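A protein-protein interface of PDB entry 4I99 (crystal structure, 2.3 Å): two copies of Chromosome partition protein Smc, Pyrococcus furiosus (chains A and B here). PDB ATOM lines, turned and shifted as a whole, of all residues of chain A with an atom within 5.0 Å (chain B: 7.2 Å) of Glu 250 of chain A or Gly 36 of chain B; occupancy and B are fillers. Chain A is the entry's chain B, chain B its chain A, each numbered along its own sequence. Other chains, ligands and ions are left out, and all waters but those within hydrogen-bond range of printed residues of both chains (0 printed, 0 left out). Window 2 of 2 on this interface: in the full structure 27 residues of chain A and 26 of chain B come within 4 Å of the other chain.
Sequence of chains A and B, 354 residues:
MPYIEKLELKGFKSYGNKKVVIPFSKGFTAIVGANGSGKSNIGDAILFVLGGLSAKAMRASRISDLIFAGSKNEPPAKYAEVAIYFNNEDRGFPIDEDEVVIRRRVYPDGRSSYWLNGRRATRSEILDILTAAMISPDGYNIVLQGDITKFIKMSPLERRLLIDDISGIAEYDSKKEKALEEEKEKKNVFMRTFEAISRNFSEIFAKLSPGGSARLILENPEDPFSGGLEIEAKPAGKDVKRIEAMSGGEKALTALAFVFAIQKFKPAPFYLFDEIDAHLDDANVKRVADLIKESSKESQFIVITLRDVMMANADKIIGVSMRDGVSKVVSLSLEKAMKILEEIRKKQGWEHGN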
ATOM      1  N   PRO A 235     -29.153 -12.725   8.459  1.00  0.00           N
ATOM      2  CA  PRO A 235     -29.933 -13.848   8.990  1.00  0.00           C
ATOM      3  C   PRO A 235     -29.537 -14.122  10.433  1.00  0.00           C
ATOM      4  O   PRO A 235     -30.394 -14.373  11.287  1.00  0.00           O
ATOM      5  CB  PRO A 235     -29.562 -15.000   8.061  1.00  0.00           C
ATOM      6  CG  PRO A 235     -29.253 -14.307   6.772  1.00  0.00           C
ATOM      7  CD  PRO A 235     -28.450 -13.115   7.225  1.00  0.00           C
ATOM      8  N   LYS A 241     -24.683 -10.836   5.329  1.00  0.00           N
ATOM      9  CA  LYS A 241     -24.524 -12.018   4.502  1.00  0.00           C
ATOM     10  C   LYS A 241     -25.006 -11.715   3.091  1.00  0.00           C
ATOM     11  O   LYS A 241     -26.108 -11.197   2.904  1.00  0.00           O
ATOM     12  CB  LYS A 241     -25.325 -13.189   5.084  1.00  0.00           C
ATOM     13  CG  LYS A 241     -25.854 -14.138   4.018  1.00  0.00           C
ATOM     14  CD  LYS A 241     -25.361 -15.566   4.164  1.00  0.00           C
ATOM     15  CE  LYS A 241     -26.177 -16.339   5.174  1.00  0.00           C
ATOM     16  NZ  LYS A 241     -25.870 -17.789   5.088  1.00  0.00           N
ATOM     17  N   ALA A 245     -25.097 -15.968  -0.893  1.00  0.00           N
ATOM     18  CA  ALA A 245     -24.431 -16.998  -0.104  1.00  0.00           C
ATOM     19  C   ALA A 245     -25.490 -17.768   0.667  1.00  0.00           C
ATOM     20  O   ALA A 245     -25.205 -18.802   1.270  1.00  0.00           O
ATOM     21  CB  ALA A 245     -23.443 -16.367   0.863  1.00  0.00           C
ATOM     22  N   MET A 246     -26.715 -17.253   0.638  1.00  0.00           N
ATOM     23  CA  MET A 246     -27.831 -17.874   1.336  1.00  0.00           C
ATOM     24  C   MET A 246     -28.211 -19.209   0.719  1.00  0.00           C
ATOM     25  O   MET A 246     -27.734 -19.567  -0.355  1.00  0.00           O
ATOM     26  CB  MET A 246     -29.053 -16.954   1.310  1.00  0.00           C
ATOM     27  CG  MET A 246     -28.869 -15.616   2.012  1.00  0.00           C
ATOM     28  SD  MET A 246     -30.533 -14.591   2.164  1.00  0.00           S
ATOM     29  CE  MET A 246     -30.848 -14.359   0.280  1.00  0.00           C
ATOM     30  N   SER A 247     -29.067 -19.947   1.418  1.00  0.00           N
ATOM     31  CA  SER A 247     -29.553 -21.234   0.938  1.00  0.00           C
ATOM     32  C   SER A 247     -30.936 -20.998   0.337  1.00  0.00           C
ATOM     33  O   SER A 247     -31.445 -19.881   0.373  1.00  0.00           O
ATOM     34  CB  SER A 247     -29.658 -22.232   2.087  1.00  0.00           C
ATOM     35  OG  SER A 247     -30.610 -21.800   3.049  1.00  0.00           O
ATOM     36  N   GLY A 248     -31.547 -22.054  -0.190  1.00  0.00           N
ATOM     37  CA  GLY A 248     -32.857 -21.926  -0.803  1.00  0.00           C
ATOM     38  C   GLY A 248     -33.929 -21.294   0.067  1.00  0.00           C
ATOM     39  O   GLY A 248     -34.657 -20.406  -0.383  1.00  0.00           O
ATOM     40  N   GLY A 249     -34.035 -21.750   1.311  1.00  0.00           N
ATOM     41  CA  GLY A 249     -35.043 -21.212   2.210  1.00  0.00           C
ATOM     42  C   GLY A 249     -34.835 -19.748   2.563  1.00  0.00           C
ATOM     43  O   GLY A 249     -35.792 -18.964   2.596  1.00  0.00           O
ATOM     44  N   GLU A 250     -33.583 -19.384   2.837  1.00  0.00           N
ATOM     45  CA  GLU A 250     -33.243 -18.015   3.190  1.00  0.00           C
ATOM     46  C   GLU A 250     -33.568 -17.091   2.033  1.00  0.00           C
ATOM     47  O   GLU A 250     -34.133 -16.015   2.225  1.00  0.00           O
ATOM     48  CB  GLU A 250     -31.761 -17.909   3.517  1.00  0.00           C
ATOM     49  CG  GLU A 250     -31.324 -18.641   4.778  1.00  0.00           C
ATOM     50  CD  GLU A 250     -29.820 -18.512   5.007  1.00  0.00           C
ATOM     51  OE1 GLU A 250     -29.049 -18.935   4.111  1.00  0.00           O
ATOM     52  OE2 GLU A 250     -29.412 -17.985   6.069  1.00  0.00           O
ATOM     53  N   LYS A 251     -33.191 -17.501   0.828  1.00  0.00           N
ATOM     54  CA  LYS A 251     -33.484 -16.699  -0.349  1.00  0.00           C
ATOM     55  C   LYS A 251     -34.995 -16.493  -0.470  1.00  0.00           C
ATOM     56  O   LYS A 251     -35.460 -15.373  -0.704  1.00  0.00           O
ATOM     57  CB  LYS A 251     -32.958 -17.374  -1.616  1.00  0.00           C
ATOM     58  CG  LYS A 251     -31.466 -17.242  -1.804  1.00  0.00           C
ATOM     59  CD  LYS A 251     -31.017 -18.019  -3.020  1.00  0.00           C
ATOM     60  CE  LYS A 251     -29.506 -17.978  -3.173  1.00  0.00           C
ATOM     61  NZ  LYS A 251     -29.061 -18.755  -4.367  1.00  0.00           N
ATOM     62  N   ALA A 252     -35.753 -17.576  -0.311  1.00  0.00           N
ATOM     63  CA  ALA A 252     -37.204 -17.505  -0.394  1.00  0.00           C
ATOM     64  C   ALA A 252     -37.754 -16.519   0.645  1.00  0.00           C
ATOM     65  O   ALA A 252     -38.600 -15.695   0.330  1.00  0.00           O
ATOM     66  CB  ALA A 252     -37.804 -18.895  -0.170  1.00  0.00           C
ATOM     67  N   LEU A 253     -37.274 -16.602   1.878  1.00  0.00           N
ATOM     68  CA  LEU A 253     -37.740 -15.705   2.925  1.00  0.00           C
ATOM     69  C   LEU A 253     -37.413 -14.256   2.615  1.00  0.00           C
ATOM     70  O   LEU A 253     -38.211 -13.358   2.883  1.00  0.00           O
ATOM     71  CB  LEU A 253     -37.120 -16.078   4.271  1.00  0.00           C
ATOM     72  CG  LEU A 253     -37.699 -17.324   4.946  1.00  0.00           C
ATOM     73  CD1 LEU A 253     -36.837 -17.695   6.152  1.00  0.00           C
ATOM     74  CD2 LEU A 253     -39.147 -17.056   5.375  1.00  0.00           C
ATOM     75  N   THR A 254     -36.235 -14.024   2.048  1.00  0.00           N
ATOM     76  CA  THR A 254     -35.833 -12.671   1.723  1.00  0.00           C
ATOM     77  C   THR A 254     -36.705 -12.110   0.608  1.00  0.00           C
ATOM     78  O   THR A 254     -37.132 -10.958   0.669  1.00  0.00           O
ATOM     79  CB  THR A 254     -34.364 -12.620   1.299  1.00  0.00           C
ATOM     80  OG1 THR A 254     -33.555 -13.178   2.344  1.00  0.00           O
ATOM     81  CG2 THR A 254     -33.940 -11.180   1.043  1.00  0.00           C
ATOM     82  N   ALA A 255     -36.974 -12.930  -0.404  1.00  0.00           N
ATOM     83  CA  ALA A 255     -37.809 -12.504  -1.519  1.00  0.00           C
ATOM     84  C   ALA A 255     -39.239 -12.249  -1.039  1.00  0.00           C
ATOM     85  O   ALA A 255     -39.871 -11.265  -1.431  1.00  0.00           O
ATOM     86  CB  ALA A 255     -37.810 -13.565  -2.618  1.00  0.00           C
ATOM     87  N   SER B  14     -20.095 -21.896   8.136  1.00  0.00           N
ATOM     88  CA  SER B  14     -20.848 -21.598   9.357  1.00  0.00           C
ATOM     89  C   SER B  14     -20.556 -22.503  10.552  1.00  0.00           C
ATOM     90  O   SER B  14     -21.131 -22.314  11.625  1.00  0.00           O
ATOM     91  CB  SER B  14     -22.351 -21.663   9.064  1.00  0.00           C
ATOM     92  OG  SER B  14     -22.743 -23.004   8.781  1.00  0.00           O
ATOM     93  N   GLY B  33     -33.061 -30.174   9.596  1.00  0.00           N
ATOM     94  CA  GLY B  33     -32.912 -29.006  10.443  1.00  0.00           C
ATOM     95  C   GLY B  33     -33.573 -27.802   9.802  1.00  0.00           C
ATOM     96  O   GLY B  33     -33.900 -27.842   8.615  1.00  0.00           O
ATOM     97  N   ALA B  34     -33.752 -26.733  10.572  1.00  0.00           N
ATOM     98  CA  ALA B  34     -34.405 -25.526  10.088  1.00  0.00           C
ATOM     99  C   ALA B  34     -33.662 -24.759   8.993  1.00  0.00           C
ATOM    100  O   ALA B  34     -32.472 -24.976   8.754  1.00  0.00           O
ATOM    101  CB  ALA B  34     -34.684 -24.597  11.259  1.00  0.00           C
ATOM    102  N   ASN B  35     -34.392 -23.867   8.321  1.00  0.00           N
ATOM    103  CA  ASN B  35     -33.823 -23.036   7.267  1.00  0.00           C
ATOM    104  C   ASN B  35     -32.696 -22.211   7.877  1.00  0.00           C
ATOM    105  O   ASN B  35     -32.838 -21.686   8.980  1.00  0.00           O
ATOM    106  CB  ASN B  35     -34.882 -22.075   6.705  1.00  0.00           C
ATOM    107  CG  ASN B  35     -35.902 -22.767   5.792  1.00  0.00           C
ATOM    108  OD1 ASN B  35     -37.057 -22.340   5.703  1.00  0.00           O
ATOM    109  ND2 ASN B  35     -35.475 -23.810   5.094  1.00  0.00           N
ATOM    110  N   GLY B  36     -31.583 -22.098   7.159  1.00  0.00           N
ATOM    111  CA  GLY B  36     -30.459 -21.307   7.640  1.00  0.00           C
ATOM    112  C   GLY B  36     -29.584 -21.957   8.695  1.00  0.00           C
ATOM    113  O   GLY B  36     -28.714 -21.299   9.260  1.00  0.00           O
ATOM    114  N   SER B  37     -29.809 -23.240   8.964  1.00  0.00           N
ATOM    115  CA  SER B  37     -29.035 -23.970   9.968  1.00  0.00           C
ATOM    116  C   SER B  37     -27.619 -24.349   9.541  1.00  0.00           C
ATOM    117  O   SER B  37     -26.744 -24.546  10.387  1.00  0.00           O
ATOM    118  CB  SER B  37     -29.775 -25.247  10.377  1.00  0.00           C
ATOM    119  OG  SER B  37     -30.915 -24.945  11.167  1.00  0.00           O
ATOM    120  N   GLY B  38     -27.400 -24.481   8.236  1.00  0.00           N
ATOM    121  CA  GLY B  38     -26.080 -24.858   7.753  1.00  0.00           C
ATOM    122  C   GLY B  38     -26.084 -26.206   7.053  1.00  0.00           C
ATOM    123  O   GLY B  38     -25.028 -26.809   6.865  1.00  0.00           O
ATOM    124  N   LYS B  39     -27.269 -26.674   6.660  1.00  0.00           N
ATOM    125  CA  LYS B  39     -27.427 -27.956   5.978  1.00  0.00           C
ATOM    126  C   LYS B  39     -26.702 -28.043   4.633  1.00  0.00           C
ATOM    127  O   LYS B  39     -25.932 -28.984   4.390  1.00  0.00           O
ATOM    128  CB  LYS B  39     -28.916 -28.267   5.755  1.00  0.00           C
ATOM    129  CG  LYS B  39     -29.689 -28.563   7.018  1.00  0.00           C
ATOM    130  CD  LYS B  39     -31.061 -29.157   6.714  1.00  0.00           C
ATOM    131  CE  LYS B  39     -31.912 -28.219   5.863  1.00  0.00           C
ATOM    132  NZ  LYS B  39     -32.075 -26.890   6.504  1.00  0.00           N
ATOM    133  N   ASN B  41     -24.356 -26.251   3.615  1.00  0.00           N
ATOM    134  CA  ASN B  41     -22.925 -26.068   3.801  1.00  0.00           C
ATOM    135  C   ASN B  41     -22.206 -27.415   3.914  1.00  0.00           C
ATOM    136  O   ASN B  41     -21.031 -27.514   3.587  1.00  0.00           O
ATOM    137  CB  ASN B  41     -22.652 -25.222   5.039  1.00  0.00           C
ATOM    138  CG  ASN B  41     -22.945 -23.762   4.803  1.00  0.00           C
ATOM    139  OD1 ASN B  41     -22.948 -23.312   3.661  1.00  0.00           O
ATOM    140  ND2 ASN B  41     -23.170 -23.010   5.874  1.00  0.00           N
ATOM    141  N   ARG B  59     -21.349 -21.427  -3.113  1.00  0.00           N
ATOM    142  CA  ARG B  59     -21.994 -20.234  -2.577  1.00  0.00           C
ATOM    143  C   ARG B  59     -21.038 -19.297  -1.855  1.00  0.00           C
ATOM    144  O   ARG B  59     -21.327 -18.834  -0.752  1.00  0.00           O
ATOM    145  CB  ARG B  59     -23.145 -20.620  -1.637  1.00  0.00           C
ATOM    146  CG  ARG B  59     -24.523 -20.748  -2.306  1.00  0.00           C
ATOM    147  CD  ARG B  59     -24.983 -22.204  -2.449  1.00  0.00           C
ATOM    148  NE  ARG B  59     -24.739 -23.021  -1.256  1.00  0.00           N
ATOM    149  CZ  ARG B  59     -25.159 -22.725  -0.024  1.00  0.00           C
ATOM    150  NH1 ARG B  59     -25.862 -21.620   0.210  1.00  0.00           N
ATOM    151  NH2 ARG B  59     -24.854 -23.529   0.986  1.00  0.00           N
ATOM    152  N   VAL B 320     -29.015 -30.721  11.981  1.00  0.00           N
ATOM    153  CA  VAL B 320     -28.210 -29.504  11.962  1.00  0.00           C
ATOM    154  C   VAL B 320     -28.939 -28.374  12.670  1.00  0.00           C
ATOM    155  O   VAL B 320     -30.130 -28.152  12.441  1.00  0.00           O
ATOM    156  CB  VAL B 320     -27.912 -29.075  10.500  1.00  0.00           C
ATOM    157  CG1 VAL B 320     -27.105 -27.788  10.465  1.00  0.00           C
ATOM    158  CG2 VAL B 320     -27.178 -30.188   9.774  1.00  0.00           C
ATOM    159  N   SER B 321     -28.232 -27.668  13.541  1.00  0.00           N
ATOM    160  CA  SER B 321     -28.820 -26.543  14.255  1.00  0.00           C
ATOM    161  C   SER B 321     -27.787 -25.451  14.454  1.00  0.00           C
ATOM    162  O   SER B 321     -26.596 -25.669  14.258  1.00  0.00           O
ATOM    163  CB  SER B 321     -29.365 -26.983  15.614  1.00  0.00           C
ATOM    164  OG  SER B 321     -28.343 -27.539  16.419  1.00  0.00           O
ATOM    165  N   MET B 322     -28.247 -24.263  14.812  1.00  0.00           N
ATOM    166  CA  MET B 322     -27.329 -23.170  15.052  1.00  0.00           C
ATOM    167  C   MET B 322     -27.260 -22.802  16.532  1.00  0.00           C
ATOM    168  O   MET B 322     -28.020 -23.311  17.357  1.00  0.00           O
ATOM    169  CB  MET B 322     -27.704 -21.942  14.229  1.00  0.00           C
ATOM    170  CG  MET B 322     -27.164 -21.964  12.818  1.00  0.00           C
ATOM    171  SD  MET B 322     -26.810 -20.171  12.163  1.00  0.00           S
ATOM    172  CE  MET B 322     -25.190 -20.528  11.173  1.00  0.00           C
ATOM    173  N   SER B 327     -23.088 -23.286  13.406  1.00  0.00           N
ATOM    174  CA  SER B 327     -23.718 -24.584  13.136  1.00  0.00           C
ATOM    175  C   SER B 327     -23.105 -25.721  13.954  1.00  0.00           C
ATOM    176  O   SER B 327     -21.947 -25.653  14.374  1.00  0.00           O
ATOM    177  CB  SER B 327     -23.612 -24.960  11.647  1.00  0.00           C
ATOM    178  OG  SER B 327     -24.130 -23.950  10.793  1.00  0.00           O
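The side-chain amide oxygen of Asn 41 of chain B is in hydrogen-bond range of the guanidinium group of Arg 59 of chain B, 3.3 Å away. The side-chain carboxylate (OE1) of Glu 250 of chain A lies within salt-bridge range of the side-chain amino group (NZ) of Lys 241 of chain A. The side-chain sulfur of Met 246 of chain A lies within hydrogen-bond range of the side-chain hydroxyl of Thr 254 of chain A (3.3 Å). N of Ser 247 of chain A is in hydrogen-bond range of OE1 of Glu 250 of chain A, 2.9 Å away. The backbone carbonyl oxygen of Glu 250 of chain A is in hydrogen-bond range of the side-chain hydroxyl of Thr 254 of chain A, at 2.9 Å.
Printed residues of chain B within 4 Å of Met 246 of chain A: Arg 59. Glu 250 of chain A touches just one residue of chain B: Gly 36 (3.8 Å). Printed residues of chain A within 4 Å of Asn 35 of chain B: Gly 249. Gly 36 of chain B touches just one residue of chain A: Glu 250. Printed residues of chain A within 4 Å of Arg 59 of chain B: Ala 245 (3.1 Å), Met 246 (2.8 Å) and Ser 247 (3.8 Å). Ser 327 of chain B touches none of the printed residues of chain A. The nearest printed residue of chain A that does not touch Arg 59 of chain B is Lys 251 of chain A (5.4 Å).
No position is printed for both chains.
Of the 14 printed residues of chain B, 3 touch a printed residue of chain A.
CA of Ser 247 of chain A touches NH1 of Arg 59 of chain B, 3.8 Å away. CA of Gly 249 of chain A touches ND2 of Asn 35 of chain B (3.9 Å). Glu 250 of chain A touches Gly 36 of chain B.
NH1 of Arg 59 of chain B lies within hydrogen-bond range of O of Ala 245 of chain A (3.1 Å). The guanidinium group of Arg 59 of chain B lies within hydrogen-bond range of the backbone carbonyl oxygen of Met 246 of chain A (2.8 Å).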
